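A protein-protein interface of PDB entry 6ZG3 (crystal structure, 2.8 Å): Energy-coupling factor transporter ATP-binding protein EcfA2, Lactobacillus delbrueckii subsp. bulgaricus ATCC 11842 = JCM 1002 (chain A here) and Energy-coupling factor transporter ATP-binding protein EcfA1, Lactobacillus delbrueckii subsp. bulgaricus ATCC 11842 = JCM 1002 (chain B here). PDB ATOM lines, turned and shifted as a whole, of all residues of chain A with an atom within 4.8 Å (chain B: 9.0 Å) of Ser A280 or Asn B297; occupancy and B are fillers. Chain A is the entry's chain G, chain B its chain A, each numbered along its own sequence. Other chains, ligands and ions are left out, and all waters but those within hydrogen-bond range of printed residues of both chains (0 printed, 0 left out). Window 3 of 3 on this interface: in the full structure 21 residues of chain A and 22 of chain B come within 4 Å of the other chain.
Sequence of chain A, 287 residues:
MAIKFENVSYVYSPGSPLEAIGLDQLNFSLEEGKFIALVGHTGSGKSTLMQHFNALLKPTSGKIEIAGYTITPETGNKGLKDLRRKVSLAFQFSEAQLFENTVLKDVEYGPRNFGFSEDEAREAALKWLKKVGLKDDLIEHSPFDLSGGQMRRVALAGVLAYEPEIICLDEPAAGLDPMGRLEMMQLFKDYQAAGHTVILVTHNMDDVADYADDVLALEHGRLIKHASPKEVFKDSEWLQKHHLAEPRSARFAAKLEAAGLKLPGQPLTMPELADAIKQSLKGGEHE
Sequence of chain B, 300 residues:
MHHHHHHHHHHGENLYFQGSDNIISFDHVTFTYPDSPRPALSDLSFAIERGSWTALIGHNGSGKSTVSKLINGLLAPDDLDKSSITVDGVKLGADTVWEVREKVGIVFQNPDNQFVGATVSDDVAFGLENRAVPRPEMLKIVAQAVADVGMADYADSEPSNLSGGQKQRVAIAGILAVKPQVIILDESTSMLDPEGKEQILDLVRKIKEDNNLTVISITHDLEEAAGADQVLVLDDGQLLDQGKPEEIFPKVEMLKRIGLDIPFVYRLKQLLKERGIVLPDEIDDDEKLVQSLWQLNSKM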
ATOM      1  N   LEU A 261      33.391 -21.532 -31.760  1.00  0.00           N
ATOM      2  CA  LEU A 261      32.739 -21.365 -30.463  1.00  0.00           C
ATOM      3  C   LEU A 261      32.678 -22.727 -29.793  1.00  0.00           C
ATOM      4  O   LEU A 261      32.304 -23.714 -30.436  1.00  0.00           O
ATOM      5  CB  LEU A 261      31.326 -20.797 -30.603  1.00  0.00           C
ATOM      6  CG  LEU A 261      31.072 -19.404 -30.045  1.00  0.00           C
ATOM      7  CD1 LEU A 261      31.461 -18.327 -31.032  1.00  0.00           C
ATOM      8  CD2 LEU A 261      29.630 -19.226 -29.605  1.00  0.00           C
ATOM      9  N   LYS A 262      33.043 -22.786 -28.511  1.00  0.00           N
ATOM     10  CA  LYS A 262      33.077 -24.065 -27.796  1.00  0.00           C
ATOM     11  C   LYS A 262      31.685 -24.377 -27.235  1.00  0.00           C
ATOM     12  O   LYS A 262      31.440 -24.382 -26.026  1.00  0.00           O
ATOM     13  CB  LYS A 262      34.162 -24.043 -26.726  1.00  0.00           C
ATOM     14  CG  LYS A 262      34.436 -25.384 -26.055  1.00  0.00           C
ATOM     15  CD  LYS A 262      35.260 -25.211 -24.785  1.00  0.00           C
ATOM     16  CE  LYS A 262      34.527 -24.432 -23.695  1.00  0.00           C
ATOM     17  NZ  LYS A 262      35.380 -24.279 -22.471  1.00  0.00           N
ATOM     18  N   LEU A 263      30.763 -24.636 -28.159  1.00  0.00           N
ATOM     19  CA  LEU A 263      29.404 -25.058 -27.820  1.00  0.00           C
ATOM     20  C   LEU A 263      29.386 -26.485 -27.292  1.00  0.00           C
ATOM     21  O   LEU A 263      29.860 -27.400 -27.981  1.00  0.00           O
ATOM     22  CB  LEU A 263      28.461 -24.933 -29.018  1.00  0.00           C
ATOM     23  CG  LEU A 263      27.667 -23.627 -29.138  1.00  0.00           C
ATOM     24  CD1 LEU A 263      28.528 -22.402 -28.977  1.00  0.00           C
ATOM     25  CD2 LEU A 263      26.901 -23.583 -30.440  1.00  0.00           C
ATOM     26  N   PRO A 264      28.862 -26.722 -26.094  1.00  0.00           N
ATOM     27  CA  PRO A 264      28.971 -28.052 -25.485  1.00  0.00           C
ATOM     28  C   PRO A 264      27.868 -28.998 -25.942  1.00  0.00           C
ATOM     29  O   PRO A 264      26.707 -28.616 -26.121  1.00  0.00           O
ATOM     30  CB  PRO A 264      28.855 -27.744 -23.987  1.00  0.00           C
ATOM     31  CG  PRO A 264      27.942 -26.535 -23.951  1.00  0.00           C
ATOM     32  CD  PRO A 264      28.267 -25.729 -25.182  1.00  0.00           C
ATOM     33  N   ALA A 276      23.456 -23.959 -24.954  1.00  0.00           N
ATOM     34  CA  ALA A 276      24.877 -24.141 -25.225  1.00  0.00           C
ATOM     35  C   ALA A 276      25.556 -22.814 -25.533  1.00  0.00           C
ATOM     36  O   ALA A 276      26.735 -22.637 -25.221  1.00  0.00           O
ATOM     37  CB  ALA A 276      25.067 -25.128 -26.375  1.00  0.00           C
ATOM     38  N   ILE A 277      24.827 -21.865 -26.124  1.00  0.00           N
ATOM     39  CA  ILE A 277      25.385 -20.535 -26.348  1.00  0.00           C
ATOM     40  C   ILE A 277      25.632 -19.841 -25.017  1.00  0.00           C
ATOM     41  O   ILE A 277      26.691 -19.243 -24.796  1.00  0.00           O
ATOM     42  CB  ILE A 277      24.449 -19.714 -27.255  1.00  0.00           C
ATOM     43  CG1 ILE A 277      24.555 -20.198 -28.709  1.00  0.00           C
ATOM     44  CG2 ILE A 277      24.718 -18.222 -27.102  1.00  0.00           C
ATOM     45  CD1 ILE A 277      23.368 -19.797 -29.575  1.00  0.00           C
ATOM     46  N   LYS A 278      24.674 -19.956 -24.097  1.00  0.00           N
ATOM     47  CA  LYS A 278      24.830 -19.370 -22.771  1.00  0.00           C
ATOM     48  C   LYS A 278      25.996 -20.018 -22.016  1.00  0.00           C
ATOM     49  O   LYS A 278      26.803 -19.323 -21.388  1.00  0.00           O
ATOM     50  CB  LYS A 278      23.522 -19.580 -21.997  1.00  0.00           C
ATOM     51  CG  LYS A 278      23.349 -18.898 -20.654  1.00  0.00           C
ATOM     52  CD  LYS A 278      23.226 -17.396 -20.720  1.00  0.00           C
ATOM     53  CE  LYS A 278      23.182 -16.826 -19.303  1.00  0.00           C
ATOM     54  NZ  LYS A 278      22.830 -15.370 -19.308  1.00  0.00           N
ATOM     55  N   GLN A 279      26.136 -21.342 -22.120  1.00  0.00           N
ATOM     56  CA  GLN A 279      27.175 -22.055 -21.380  1.00  0.00           C
ATOM     57  C   GLN A 279      28.553 -21.815 -21.977  1.00  0.00           C
ATOM     58  O   GLN A 279      29.544 -21.726 -21.245  1.00  0.00           O
ATOM     59  CB  GLN A 279      26.870 -23.550 -21.340  1.00  0.00           C
ATOM     60  CG  GLN A 279      26.724 -24.135 -19.925  1.00  0.00           C
ATOM     61  CD  GLN A 279      28.071 -24.279 -19.223  1.00  0.00           C
ATOM     62  OE1 GLN A 279      29.085 -24.552 -19.871  1.00  0.00           O
ATOM     63  NE2 GLN A 279      28.089 -24.099 -17.904  1.00  0.00           N
ATOM     64  N   SER A 280      28.622 -21.662 -23.299  1.00  0.00           N
ATOM     65  CA  SER A 280      29.855 -21.322 -23.992  1.00  0.00           C
ATOM     66  C   SER A 280      30.269 -19.876 -23.806  1.00  0.00           C
ATOM     67  O   SER A 280      31.457 -19.581 -23.934  1.00  0.00           O
ATOM     68  CB  SER A 280      29.701 -21.614 -25.483  1.00  0.00           C
ATOM     69  OG  SER A 280      30.926 -21.444 -26.164  1.00  0.00           O
ATOM     70  N   LEU A 281      29.339 -18.965 -23.504  1.00  0.00           N
ATOM     71  CA  LEU A 281      29.742 -17.565 -23.439  1.00  0.00           C
ATOM     72  C   LEU A 281      30.646 -17.298 -22.247  1.00  0.00           C
ATOM     73  O   LEU A 281      31.735 -16.736 -22.410  1.00  0.00           O
ATOM     74  CB  LEU A 281      28.532 -16.632 -23.398  1.00  0.00           C
ATOM     75  CG  LEU A 281      27.715 -16.318 -24.654  1.00  0.00           C
ATOM     76  CD1 LEU A 281      27.050 -14.960 -24.493  1.00  0.00           C
ATOM     77  CD2 LEU A 281      28.570 -16.334 -25.902  1.00  0.00           C
ATOM     78  N   LYS A 282      30.226 -17.675 -21.043  1.00  0.00           N
ATOM     79  CA  LYS A 282      31.094 -17.575 -19.870  1.00  0.00           C
ATOM     80  C   LYS A 282      31.793 -18.920 -19.653  1.00  0.00           C
ATOM     81  O   LYS A 282      31.132 -19.959 -19.534  1.00  0.00           O
ATOM     82  CB  LYS A 282      30.312 -17.109 -18.636  1.00  0.00           C
ATOM     83  CG  LYS A 282      29.513 -18.152 -17.867  1.00  0.00           C
ATOM     84  CD  LYS A 282      28.349 -18.712 -18.658  1.00  0.00           C
ATOM     85  CE  LYS A 282      27.963 -20.074 -18.102  1.00  0.00           C
ATOM     86  NZ  LYS A 282      29.132 -21.003 -18.032  1.00  0.00           N
ATOM     87  N   GLY A 283      33.126 -18.905 -19.648  1.00  0.00           N
ATOM     88  CA  GLY A 283      33.905 -20.124 -19.457  1.00  0.00           C
ATOM     89  C   GLY A 283      33.640 -21.242 -20.461  1.00  0.00           C
ATOM     90  O   GLY A 283      33.656 -22.431 -20.119  1.00  0.00           O
ATOM     91  N   ILE B 277      21.024 -13.330 -22.149  1.00  0.00           N
ATOM     92  CA  ILE B 277      21.834 -12.731 -23.204  1.00  0.00           C
ATOM     93  C   ILE B 277      20.912 -11.892 -24.080  1.00  0.00           C
ATOM     94  O   ILE B 277      20.022 -12.423 -24.748  1.00  0.00           O
ATOM     95  CB  ILE B 277      22.540 -13.814 -24.037  1.00  0.00           C
ATOM     96  CG1 ILE B 277      23.280 -14.810 -23.147  1.00  0.00           C
ATOM     97  CG2 ILE B 277      23.489 -13.187 -25.020  1.00  0.00           C
ATOM     98  CD1 ILE B 277      23.772 -16.040 -23.889  1.00  0.00           C
ATOM     99  N   VAL B 290      26.142 -14.744 -36.059  1.00  0.00           N
ATOM    100  CA  VAL B 290      27.357 -15.507 -35.816  1.00  0.00           C
ATOM    101  C   VAL B 290      28.467 -14.564 -35.424  1.00  0.00           C
ATOM    102  O   VAL B 290      29.181 -14.790 -34.442  1.00  0.00           O
ATOM    103  CB  VAL B 290      27.747 -16.346 -37.042  1.00  0.00           C
ATOM    104  CG1 VAL B 290      29.229 -16.623 -37.014  1.00  0.00           C
ATOM    105  CG2 VAL B 290      26.999 -17.663 -37.050  1.00  0.00           C
ATOM    106  N   GLN B 291      28.601 -13.465 -36.159  1.00  0.00           N
ATOM    107  CA  GLN B 291      29.648 -12.517 -35.805  1.00  0.00           C
ATOM    108  C   GLN B 291      29.414 -11.929 -34.420  1.00  0.00           C
ATOM    109  O   GLN B 291      30.368 -11.668 -33.680  1.00  0.00           O
ATOM    110  CB  GLN B 291      29.736 -11.392 -36.821  1.00  0.00           C
ATOM    111  CG  GLN B 291      31.115 -10.823 -36.935  1.00  0.00           C
ATOM    112  CD  GLN B 291      31.055  -9.456 -37.495  1.00  0.00           C
ATOM    113  OE1 GLN B 291      30.034  -9.050 -38.031  1.00  0.00           O
ATOM    114  NE2 GLN B 291      32.143  -8.727 -37.391  1.00  0.00           N
ATOM    115  N   SER B 292      28.155 -11.694 -34.057  1.00  0.00           N
ATOM    116  CA  SER B 292      27.867 -11.110 -32.752  1.00  0.00           C
ATOM    117  C   SER B 292      28.326 -12.017 -31.616  1.00  0.00           C
ATOM    118  O   SER B 292      29.075 -11.601 -30.724  1.00  0.00           O
ATOM    119  CB  SER B 292      26.374 -10.832 -32.630  1.00  0.00           C
ATOM    120  OG  SER B 292      26.084 -10.192 -31.401  1.00  0.00           O
ATOM    121  N   LEU B 293      27.873 -13.266 -31.629  1.00  0.00           N
ATOM    122  CA  LEU B 293      28.285 -14.208 -30.589  1.00  0.00           C
ATOM    123  C   LEU B 293      29.798 -14.468 -30.618  1.00  0.00           C
ATOM    124  O   LEU B 293      30.434 -14.610 -29.556  1.00  0.00           O
ATOM    125  CB  LEU B 293      27.479 -15.495 -30.749  1.00  0.00           C
ATOM    126  CG  LEU B 293      25.962 -15.293 -30.651  1.00  0.00           C
ATOM    127  CD1 LEU B 293      25.282 -16.480 -31.284  1.00  0.00           C
ATOM    128  CD2 LEU B 293      25.468 -15.077 -29.207  1.00  0.00           C
ATOM    129  N   TRP B 294      30.394 -14.492 -31.814  1.00  0.00           N
ATOM    130  CA  TRP B 294      31.844 -14.532 -31.944  1.00  0.00           C
ATOM    131  C   TRP B 294      32.478 -13.419 -31.145  1.00  0.00           C
ATOM    132  O   TRP B 294      33.412 -13.637 -30.368  1.00  0.00           O
ATOM    133  CB  TRP B 294      32.242 -14.349 -33.407  1.00  0.00           C
ATOM    134  CG  TRP B 294      33.737 -14.303 -33.633  1.00  0.00           C
ATOM    135  CD1 TRP B 294      34.571 -13.229 -33.435  1.00  0.00           C
ATOM    136  CD2 TRP B 294      34.548 -15.319 -34.239  1.00  0.00           C
ATOM    137  NE1 TRP B 294      35.854 -13.550 -33.796  1.00  0.00           N
ATOM    138  CE2 TRP B 294      35.865 -14.820 -34.305  1.00  0.00           C
ATOM    139  CE3 TRP B 294      34.298 -16.606 -34.703  1.00  0.00           C
ATOM    140  CZ2 TRP B 294      36.920 -15.570 -34.814  1.00  0.00           C
ATOM    141  CZ3 TRP B 294      35.345 -17.346 -35.222  1.00  0.00           C
ATOM    142  CH2 TRP B 294      36.640 -16.836 -35.261  1.00  0.00           C
ATOM    143  N   GLN B 295      32.000 -12.200 -31.372  1.00  0.00           N
ATOM    144  CA  GLN B 295      32.597 -11.048 -30.729  1.00  0.00           C
ATOM    145  C   GLN B 295      32.346 -11.058 -29.225  1.00  0.00           C
ATOM    146  O   GLN B 295      33.171 -10.539 -28.464  1.00  0.00           O
ATOM    147  CB  GLN B 295      32.059  -9.781 -31.386  1.00  0.00           C
ATOM    148  CG  GLN B 295      32.924  -8.538 -31.215  1.00  0.00           C
ATOM    149  CD  GLN B 295      32.383  -7.598 -30.147  1.00  0.00           C
ATOM    150  OE1 GLN B 295      31.544  -7.985 -29.325  1.00  0.00           O
ATOM    151  NE2 GLN B 295      32.847  -6.353 -30.164  1.00  0.00           N
ATOM    152  N   LEU B 296      31.240 -11.653 -28.770  1.00  0.00           N
ATOM    153  CA  LEU B 296      31.038 -11.773 -27.324  1.00  0.00           C
ATOM    154  C   LEU B 296      32.024 -12.725 -26.664  1.00  0.00           C
ATOM    155  O   LEU B 296      32.501 -12.448 -25.559  1.00  0.00           O
ATOM    156  CB  LEU B 296      29.617 -12.209 -26.981  1.00  0.00           C
ATOM    157  CG  LEU B 296      28.610 -11.093 -26.722  1.00  0.00           C
ATOM    158  CD1 LEU B 296      28.245 -10.326 -27.978  1.00  0.00           C
ATOM    159  CD2 LEU B 296      27.388 -11.670 -26.037  1.00  0.00           C
ATOM    160  N   ASN B 297      32.369 -13.838 -27.311  1.00  0.00           N
ATOM    161  CA  ASN B 297      33.274 -14.741 -26.603  1.00  0.00           C
ATOM    162  C   ASN B 297      34.695 -14.230 -26.458  1.00  0.00           C
ATOM    163  O   ASN B 297      35.392 -14.665 -25.535  1.00  0.00           O
ATOM    164  CB  ASN B 297      33.273 -16.124 -27.225  1.00  0.00           C
ATOM    165  CG  ASN B 297      32.069 -16.895 -26.811  1.00  0.00           C
ATOM    166  OD1 ASN B 297      31.625 -16.769 -25.672  1.00  0.00           O
ATOM    167  ND2 ASN B 297      31.529 -17.686 -27.697  1.00  0.00           N
ATOM    168  N   SER B 298      35.155 -13.338 -27.323  1.00  0.00           N
ATOM    169  CA  SER B 298      36.523 -12.856 -27.172  1.00  0.00           C
ATOM    170  C   SER B 298      36.611 -11.912 -25.966  1.00  0.00           C
ATOM    171  O   SER B 298      37.659 -11.835 -25.313  1.00  0.00           O
ATOM    172  CB  SER B 298      36.998 -12.153 -28.444  1.00  0.00           C
ATOM    173  OG  SER B 298      36.521 -10.820 -28.491  1.00  0.00           O
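Leu A261 touches Trp B294 (CD1 to CA, 3.9 Å). Leu A261 touches Asn B297 (CG to ND2, 2.9 Å). CD1 of Ile B277 touches CG2 of Ile A277 (3.997 Å). Ile A277 touches Leu B293 (CG2 to CD2, 3.9 Å). Ile B277 touches Lys A278. Leu A281 touches Ile B277 (CD1 to CD1, 3.5 Å). CD2 of Leu B296 touches CD1 of Leu A281, at 3.6 Å.
OG of Ser A280 lies within hydrogen-bond range of O of Lys A262.
Asn B297 touches just these residues of chain A: Leu A261, Ser A280 and Leu A281. Printed residues of chain B within 4 Å of Leu A261: Trp B294 (3.9 Å) and Asn B297 (2.9 Å). Of the printed residues of chain B, Leu A281 touches Ile B277 (3.5 Å), Leu B296 (3.6 Å) and Asn B297 (3.0 Å). Of the printed residues of chain B, Lys A278 touches Ile B277 (3.5 Å). Printed residues of chain A within 4 Å of Leu B296: Leu A281.
Of the 10 printed residues of chain B, 5 touch a printed residue of chain A. Hydrophobic or aromatic side chains of chain B that line the printed part of chain A: Ile B277, Leu B293 and Leu B296. Printed residues of chain A that touch a printed residue of chain B: Leu A261, Ile A277, Lys A278, Ser A280 and Leu A281. Hydrophobic or aromatic side chains of chain A that line the printed part of chain B: Leu A261, Ile A277 and Leu A281. Among the printed residues, no Asp or Glu carboxylate lies within 4 Å of a Lys or Arg side-chain nitrogen of the other chain.
The side-chain amide oxygen of Asn B297 lies close to the backbone carbonyl oxygen of Ser A280 (3.3 Å). The side-chain amide oxygen (OD1) of Asn B297 lies close to the backbone carbonyl oxygen (O) of Leu A281, at 3.3 Å.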
